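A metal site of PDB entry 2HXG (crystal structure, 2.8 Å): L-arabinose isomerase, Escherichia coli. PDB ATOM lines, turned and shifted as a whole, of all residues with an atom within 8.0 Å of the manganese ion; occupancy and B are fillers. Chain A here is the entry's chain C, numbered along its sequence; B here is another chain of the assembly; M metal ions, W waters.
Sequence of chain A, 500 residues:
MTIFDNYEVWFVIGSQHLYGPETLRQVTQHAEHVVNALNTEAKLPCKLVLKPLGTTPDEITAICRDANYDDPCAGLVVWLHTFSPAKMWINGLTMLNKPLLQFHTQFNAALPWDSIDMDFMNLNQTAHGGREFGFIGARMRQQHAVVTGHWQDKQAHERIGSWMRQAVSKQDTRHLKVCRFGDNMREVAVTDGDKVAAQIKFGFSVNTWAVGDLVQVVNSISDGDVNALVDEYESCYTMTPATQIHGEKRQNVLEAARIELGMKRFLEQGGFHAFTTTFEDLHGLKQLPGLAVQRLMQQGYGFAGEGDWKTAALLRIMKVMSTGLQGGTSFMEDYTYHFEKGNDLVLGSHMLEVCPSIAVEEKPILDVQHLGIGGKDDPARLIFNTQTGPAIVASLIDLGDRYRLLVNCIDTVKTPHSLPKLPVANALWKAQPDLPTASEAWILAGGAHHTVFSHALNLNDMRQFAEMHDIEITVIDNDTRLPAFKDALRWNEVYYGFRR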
ATOM      1  N   MET A 185      12.319   1.175 -14.040  1.00  0.00           N
ATOM      2  CA  MET A 185      12.132   0.155 -15.070  1.00  0.00           C
ATOM      3  C   MET A 185      13.462  -0.599 -15.164  1.00  0.00           C
ATOM      4  O   MET A 185      14.524   0.011 -15.080  1.00  0.00           O
ATOM      5  CB  MET A 185      11.797   0.807 -16.419  1.00  0.00           C
ATOM      6  CG  MET A 185      10.794   0.069 -17.293  1.00  0.00           C
ATOM      7  SD  MET A 185      11.224   0.209 -19.050  1.00  0.00           S
ATOM      8  CE  MET A 185      11.214   1.979 -19.329  1.00  0.00           C
ATOM      9  N   VAL A 188      17.003  -0.268 -17.894  1.00  0.00           N
ATOM     10  CA  VAL A 188      17.188   1.124 -18.325  1.00  0.00           C
ATOM     11  C   VAL A 188      18.427   1.660 -17.596  1.00  0.00           C
ATOM     12  O   VAL A 188      18.852   1.070 -16.595  1.00  0.00           O
ATOM     13  CB  VAL A 188      15.952   2.035 -18.024  1.00  0.00           C
ATOM     14  CG1 VAL A 188      15.730   3.047 -19.141  1.00  0.00           C
ATOM     15  CG2 VAL A 188      14.692   1.240 -17.880  1.00  0.00           C
ATOM     16  N   THR A 191      17.770   6.621 -16.457  1.00  0.00           N
ATOM     17  CA  THR A 191      16.810   6.904 -15.366  1.00  0.00           C
ATOM     18  C   THR A 191      17.433   6.645 -13.984  1.00  0.00           C
ATOM     19  O   THR A 191      16.988   7.221 -12.981  1.00  0.00           O
ATOM     20  CB  THR A 191      15.478   6.063 -15.472  1.00  0.00           C
ATOM     21  OG1 THR A 191      15.435   5.073 -14.441  1.00  0.00           O
ATOM     22  CG2 THR A 191      15.323   5.366 -16.816  1.00  0.00           C
ATOM     23  N   THR A 277       6.161   6.132 -10.955  1.00  0.00           N
ATOM     24  CA  THR A 277       5.484   4.831 -11.015  1.00  0.00           C
ATOM     25  C   THR A 277       6.086   3.943 -12.105  1.00  0.00           C
ATOM     26  O   THR A 277       6.331   4.402 -13.211  1.00  0.00           O
ATOM     27  CB  THR A 277       3.954   4.966 -11.263  1.00  0.00           C
ATOM     28  OG1 THR A 277       3.573   4.105 -12.350  1.00  0.00           O
ATOM     29  CG2 THR A 277       3.562   6.384 -11.644  1.00  0.00           C
ATOM     30  N   PHE A 279       5.494   0.628 -14.424  1.00  0.00           N
ATOM     31  CA  PHE A 279       4.512  -0.363 -14.931  1.00  0.00           C
ATOM     32  C   PHE A 279       4.963  -1.807 -14.675  1.00  0.00           C
ATOM     33  O   PHE A 279       4.138  -2.715 -14.602  1.00  0.00           O
ATOM     34  CB  PHE A 279       4.208  -0.149 -16.423  1.00  0.00           C
ATOM     35  CG  PHE A 279       5.416  -0.218 -17.313  1.00  0.00           C
ATOM     36  CD1 PHE A 279       6.058  -1.438 -17.545  1.00  0.00           C
ATOM     37  CD2 PHE A 279       5.906   0.913 -17.938  1.00  0.00           C
ATOM     38  CE1 PHE A 279       7.161  -1.504 -18.373  1.00  0.00           C
ATOM     39  CE2 PHE A 279       7.022   0.841 -18.776  1.00  0.00           C
ATOM     40  CZ  PHE A 279       7.644  -0.375 -18.986  1.00  0.00           C
ATOM     41  N   ALA A 304       7.520  11.801 -13.296  1.00  0.00           N
ATOM     42  CA  ALA A 304       8.164  11.364 -14.529  1.00  0.00           C
ATOM     43  C   ALA A 304       7.821   9.904 -14.763  1.00  0.00           C
ATOM     44  O   ALA A 304       6.958   9.352 -14.072  1.00  0.00           O
ATOM     45  CB  ALA A 304       9.659  11.567 -14.426  1.00  0.00           C
ATOM     46  N   GLY A 305       8.501   9.262 -15.710  1.00  0.00           N
ATOM     47  CA  GLY A 305       8.125   7.922 -16.165  1.00  0.00           C
ATOM     48  C   GLY A 305       8.372   6.771 -15.190  1.00  0.00           C
ATOM     49  O   GLY A 305       7.858   6.772 -14.071  1.00  0.00           O
ATOM     50  N   GLU A 306       9.148   5.795 -15.632  1.00  0.00           N
ATOM     51  CA  GLU A 306       9.273   4.533 -14.932  1.00  0.00           C
ATOM     52  C   GLU A 306      10.423   4.601 -13.940  1.00  0.00           C
ATOM     53  O   GLU A 306      11.520   4.112 -14.205  1.00  0.00           O
ATOM     54  CB  GLU A 306       9.462   3.398 -15.934  1.00  0.00           C
ATOM     55  CG  GLU A 306       8.268   3.190 -16.897  1.00  0.00           C
ATOM     56  CD  GLU A 306       8.328   4.035 -18.180  1.00  0.00           C
ATOM     57  OE1 GLU A 306       9.339   4.706 -18.459  1.00  0.00           O
ATOM     58  OE2 GLU A 306       7.330   4.011 -18.941  1.00  0.00           O
ATOM     59  N   GLY A 307      10.135   5.236 -12.811  1.00  0.00           N
ATOM     60  CA  GLY A 307      11.101   5.416 -11.726  1.00  0.00           C
ATOM     61  C   GLY A 307      12.078   6.562 -11.939  1.00  0.00           C
ATOM     62  O   GLY A 307      13.018   6.719 -11.153  1.00  0.00           O
ATOM     63  N   ASP A 308      11.876   7.360 -12.980  1.00  0.00           N
ATOM     64  CA  ASP A 308      12.807   8.430 -13.338  1.00  0.00           C
ATOM     65  C   ASP A 308      12.651   9.613 -12.389  1.00  0.00           C
ATOM     66  O   ASP A 308      11.970  10.603 -12.685  1.00  0.00           O
ATOM     67  CB  ASP A 308      12.610   8.862 -14.788  1.00  0.00           C
ATOM     68  CG  ASP A 308      13.578   9.970 -15.207  1.00  0.00           C
ATOM     69  OD1 ASP A 308      14.623  10.189 -14.526  1.00  0.00           O
ATOM     70  OD2 ASP A 308      13.285  10.623 -16.235  1.00  0.00           O
ATOM     71  N   PHE A 331       5.603  17.152 -18.093  1.00  0.00           N
ATOM     72  CA  PHE A 331       6.536  16.057 -18.328  1.00  0.00           C
ATOM     73  C   PHE A 331       6.361  15.664 -19.783  1.00  0.00           C
ATOM     74  O   PHE A 331       5.284  15.868 -20.359  1.00  0.00           O
ATOM     75  CB  PHE A 331       6.225  14.889 -17.390  1.00  0.00           C
ATOM     76  CG  PHE A 331       6.749  13.564 -17.857  1.00  0.00           C
ATOM     77  CD1 PHE A 331       8.103  13.302 -17.842  1.00  0.00           C
ATOM     78  CD2 PHE A 331       5.884  12.579 -18.296  1.00  0.00           C
ATOM     79  CE1 PHE A 331       8.591  12.077 -18.270  1.00  0.00           C
ATOM     80  CE2 PHE A 331       6.359  11.359 -18.714  1.00  0.00           C
ATOM     81  CZ  PHE A 331       7.721  11.100 -18.711  1.00  0.00           C
ATOM     82  N   MET A 332       7.411  15.112 -20.389  1.00  0.00           N
ATOM     83  CA  MET A 332       7.360  14.759 -21.813  1.00  0.00           C
ATOM     84  C   MET A 332       8.464  13.785 -22.190  1.00  0.00           C
ATOM     85  O   MET A 332       9.515  13.770 -21.561  1.00  0.00           O
ATOM     86  CB  MET A 332       7.502  16.037 -22.648  1.00  0.00           C
ATOM     87  CG  MET A 332       7.277  15.866 -24.135  1.00  0.00           C
ATOM     88  SD  MET A 332       5.545  15.736 -24.561  1.00  0.00           S
ATOM     89  CE  MET A 332       4.997  17.414 -24.254  1.00  0.00           C
ATOM     90  N   GLU A 333       8.199  12.955 -23.193  1.00  0.00           N
ATOM     91  CA  GLU A 333       9.268  12.292 -23.956  1.00  0.00           C
ATOM     92  C   GLU A 333       8.976  12.338 -25.451  1.00  0.00           C
ATOM     93  O   GLU A 333       7.827  12.505 -25.861  1.00  0.00           O
ATOM     94  CB  GLU A 333       9.568  10.864 -23.481  1.00  0.00           C
ATOM     95  CG  GLU A 333       8.426   9.866 -23.489  1.00  0.00           C
ATOM     96  CD  GLU A 333       8.889   8.457 -23.077  1.00  0.00           C
ATOM     97  OE1 GLU A 333       9.371   7.717 -23.955  1.00  0.00           O
ATOM     98  OE2 GLU A 333       8.772   8.092 -21.890  1.00  0.00           O
ATOM     99  N   SER A 349       4.978  12.818 -26.236  1.00  0.00           N
ATOM    100  CA  SER A 349       3.871  12.335 -25.407  1.00  0.00           C
ATOM    101  C   SER A 349       4.423  11.384 -24.338  1.00  0.00           C
ATOM    102  O   SER A 349       5.599  11.460 -23.983  1.00  0.00           O
ATOM    103  CB  SER A 349       2.809  11.612 -26.246  1.00  0.00           C
ATOM    104  OG  SER A 349       1.771  11.110 -25.421  1.00  0.00           O
ATOM    105  N   HIS A 350       3.572  10.494 -23.835  1.00  0.00           N
ATOM    106  CA  HIS A 350       4.026   9.379 -23.003  1.00  0.00           C
ATOM    107  C   HIS A 350       2.977   8.262 -23.001  1.00  0.00           C
ATOM    108  O   HIS A 350       1.830   8.465 -23.417  1.00  0.00           O
ATOM    109  CB  HIS A 350       4.307   9.844 -21.573  1.00  0.00           C
ATOM    110  CG  HIS A 350       5.057   8.846 -20.742  1.00  0.00           C
ATOM    111  ND1 HIS A 350       4.423   7.862 -20.014  1.00  0.00           N
ATOM    112  CD2 HIS A 350       6.380   8.666 -20.544  1.00  0.00           C
ATOM    113  CE1 HIS A 350       5.334   7.123 -19.389  1.00  0.00           C
ATOM    114  NE2 HIS A 350       6.523   7.592 -19.694  1.00  0.00           N
ATOM    115  N   MET A 351       3.418   7.087 -22.566  1.00  0.00           N
ATOM    116  CA  MET A 351       2.550   5.944 -22.273  1.00  0.00           C
ATOM    117  C   MET A 351       1.122   6.338 -21.833  1.00  0.00           C
ATOM    118  O   MET A 351       0.141   5.770 -22.310  1.00  0.00           O
ATOM    119  CB  MET A 351       3.225   5.066 -21.200  1.00  0.00           C
ATOM    120  CG  MET A 351       2.879   3.585 -21.277  1.00  0.00           C
ATOM    121  SD  MET A 351       3.740   2.526 -20.081  1.00  0.00           S
ATOM    122  CE  MET A 351       3.030   3.107 -18.549  1.00  0.00           C
ATOM    123  N   GLU A 353       0.714   9.824 -19.593  1.00  0.00           N
ATOM    124  CA  GLU A 353       0.670  10.975 -18.692  1.00  0.00           C
ATOM    125  C   GLU A 353       1.372  12.240 -19.231  1.00  0.00           C
ATOM    126  O   GLU A 353       2.581  12.408 -19.079  1.00  0.00           O
ATOM    127  CB  GLU A 353       1.274  10.598 -17.328  1.00  0.00           C
ATOM    128  CG  GLU A 353       1.174   9.100 -16.950  1.00  0.00           C
ATOM    129  CD  GLU A 353       2.295   8.242 -17.543  1.00  0.00           C
ATOM    130  OE1 GLU A 353       3.198   8.798 -18.198  1.00  0.00           O
ATOM    131  OE2 GLU A 353       2.277   7.006 -17.341  1.00  0.00           O
ATOM    132  N   HIS A 449      15.773  10.748 -22.833  1.00  0.00           N
ATOM    133  CA  HIS A 449      14.578  10.740 -23.656  1.00  0.00           C
ATOM    134  C   HIS A 449      13.393  11.421 -22.955  1.00  0.00           C
ATOM    135  O   HIS A 449      12.530  11.997 -23.619  1.00  0.00           O
ATOM    136  CB  HIS A 449      14.229   9.320 -24.141  1.00  0.00           C
ATOM    137  CG  HIS A 449      13.762   8.377 -23.061  1.00  0.00           C
ATOM    138  ND1 HIS A 449      14.615   7.835 -22.126  1.00  0.00           N
ATOM    139  CD2 HIS A 449      12.546   7.826 -22.830  1.00  0.00           C
ATOM    140  CE1 HIS A 449      13.935   7.016 -21.338  1.00  0.00           C
ATOM    141  NE2 HIS A 449      12.678   7.003 -21.746  1.00  0.00           N
ATOM    142  N   HIS A 450      13.375  11.386 -21.620  1.00  0.00           N
ATOM    143  CA  HIS A 450      12.425  12.179 -20.832  1.00  0.00           C
ATOM    144  C   HIS A 450      12.881  13.631 -20.752  1.00  0.00           C
ATOM    145  O   HIS A 450      14.073  13.926 -20.733  1.00  0.00           O
ATOM    146  CB  HIS A 450      12.259  11.610 -19.420  1.00  0.00           C
ATOM    147  CG  HIS A 450      11.671  10.233 -19.375  1.00  0.00           C
ATOM    148  ND1 HIS A 450      11.618   9.470 -18.229  1.00  0.00           N
ATOM    149  CD2 HIS A 450      11.152   9.465 -20.360  1.00  0.00           C
ATOM    150  CE1 HIS A 450      11.075   8.307 -18.501  1.00  0.00           C
ATOM    151  NE2 HIS A 450      10.781   8.269 -19.788  1.00  0.00           N
ATOM    152  N   PHE B  83      13.129  -0.279 -28.703  1.00  0.00           N
ATOM    153  CA  PHE B  83      13.627   0.417 -27.510  1.00  0.00           C
ATOM    154  C   PHE B  83      14.497  -0.603 -26.781  1.00  0.00           C
ATOM    155  O   PHE B  83      13.976  -1.602 -26.277  1.00  0.00           O
ATOM    156  CB  PHE B  83      12.476   0.906 -26.606  1.00  0.00           C
ATOM    157  CG  PHE B  83      12.944   1.550 -25.299  1.00  0.00           C
ATOM    158  CD1 PHE B  83      12.472   1.086 -24.064  1.00  0.00           C
ATOM    159  CD2 PHE B  83      13.824   2.614 -25.303  1.00  0.00           C
ATOM    160  CE1 PHE B  83      12.890   1.677 -22.865  1.00  0.00           C
ATOM    161  CE2 PHE B  83      14.251   3.210 -24.105  1.00  0.00           C
ATOM    162  CZ  PHE B  83      13.776   2.743 -22.891  1.00  0.00           C
ATOM    163  N   HIS B 128      12.804   8.065 -28.830  1.00  0.00           N
ATOM    164  CA  HIS B 128      13.266   7.969 -27.436  1.00  0.00           C
ATOM    165  C   HIS B 128      14.374   6.936 -27.283  1.00  0.00           C
ATOM    166  O   HIS B 128      15.404   7.220 -26.672  1.00  0.00           O
ATOM    167  CB  HIS B 128      12.104   7.752 -26.432  1.00  0.00           C
ATOM    168  CG  HIS B 128      11.144   6.671 -26.803  1.00  0.00           C
ATOM    169  ND1 HIS B 128      10.004   6.901 -27.551  1.00  0.00           N
ATOM    170  CD2 HIS B 128      11.105   5.355 -26.473  1.00  0.00           C
ATOM    171  CE1 HIS B 128       9.339   5.772 -27.703  1.00  0.00           C
ATOM    172  NE2 HIS B 128       9.980   4.819 -27.052  1.00  0.00           N
HETATM  173 MN    MN M   1       9.092   6.208 -20.432  1.00  0.00          MN
HETATM  174  O   HOH W   1      10.792   5.106 -21.711  1.00  0.00           O
HETATM  175  O   HOH W   2       8.397   5.391 -22.674  1.00  0.00           O
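The side-chain carboxylate (OE2) of Glu 333 lies close to a ring nitrogen (NE2) of His 350, 3.2 Å away.
The backbone carbonyl oxygen (O) of Glu 333 sits at hydrogen-bond distance from the backbone NH (N) of Ser 349.
The backbone carbonyl oxygen (O) of Glu 306 sits at hydrogen-bond distance from the backbone NH (N) of Met 185 (3.0 Å).
A ring nitrogen (NE2) of His 450 sits close to a ring nitrogen (NE2) of His 449, 3.0 Å away.
ND1 of His 450 lies within hydrogen-bond range of OD2 of Asp 308, at 2.8 Å.
The manganese ion is bound by water W1 (2.4 Å).
OE2 of Glu 333 is bound to the manganese ion, 2.4 Å away.
Water W2 is bound to the manganese ion, at 2.5 Å.
OE1 of Glu 306 binds the manganese ion (2.5 Å).
A ring nitrogen (NE2) of His 450 is bound to the manganese ion, at 2.7 Å.
The manganese ion has five donor atoms within binding distance.
Merely in contact with the manganese ion: His 350 (3.0 Å) and His 449 (3.9 Å).
Five residues have an atom within 4 Å of the manganese ion: Glu 306, Glu 333, His 350, His 449 and His 450.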
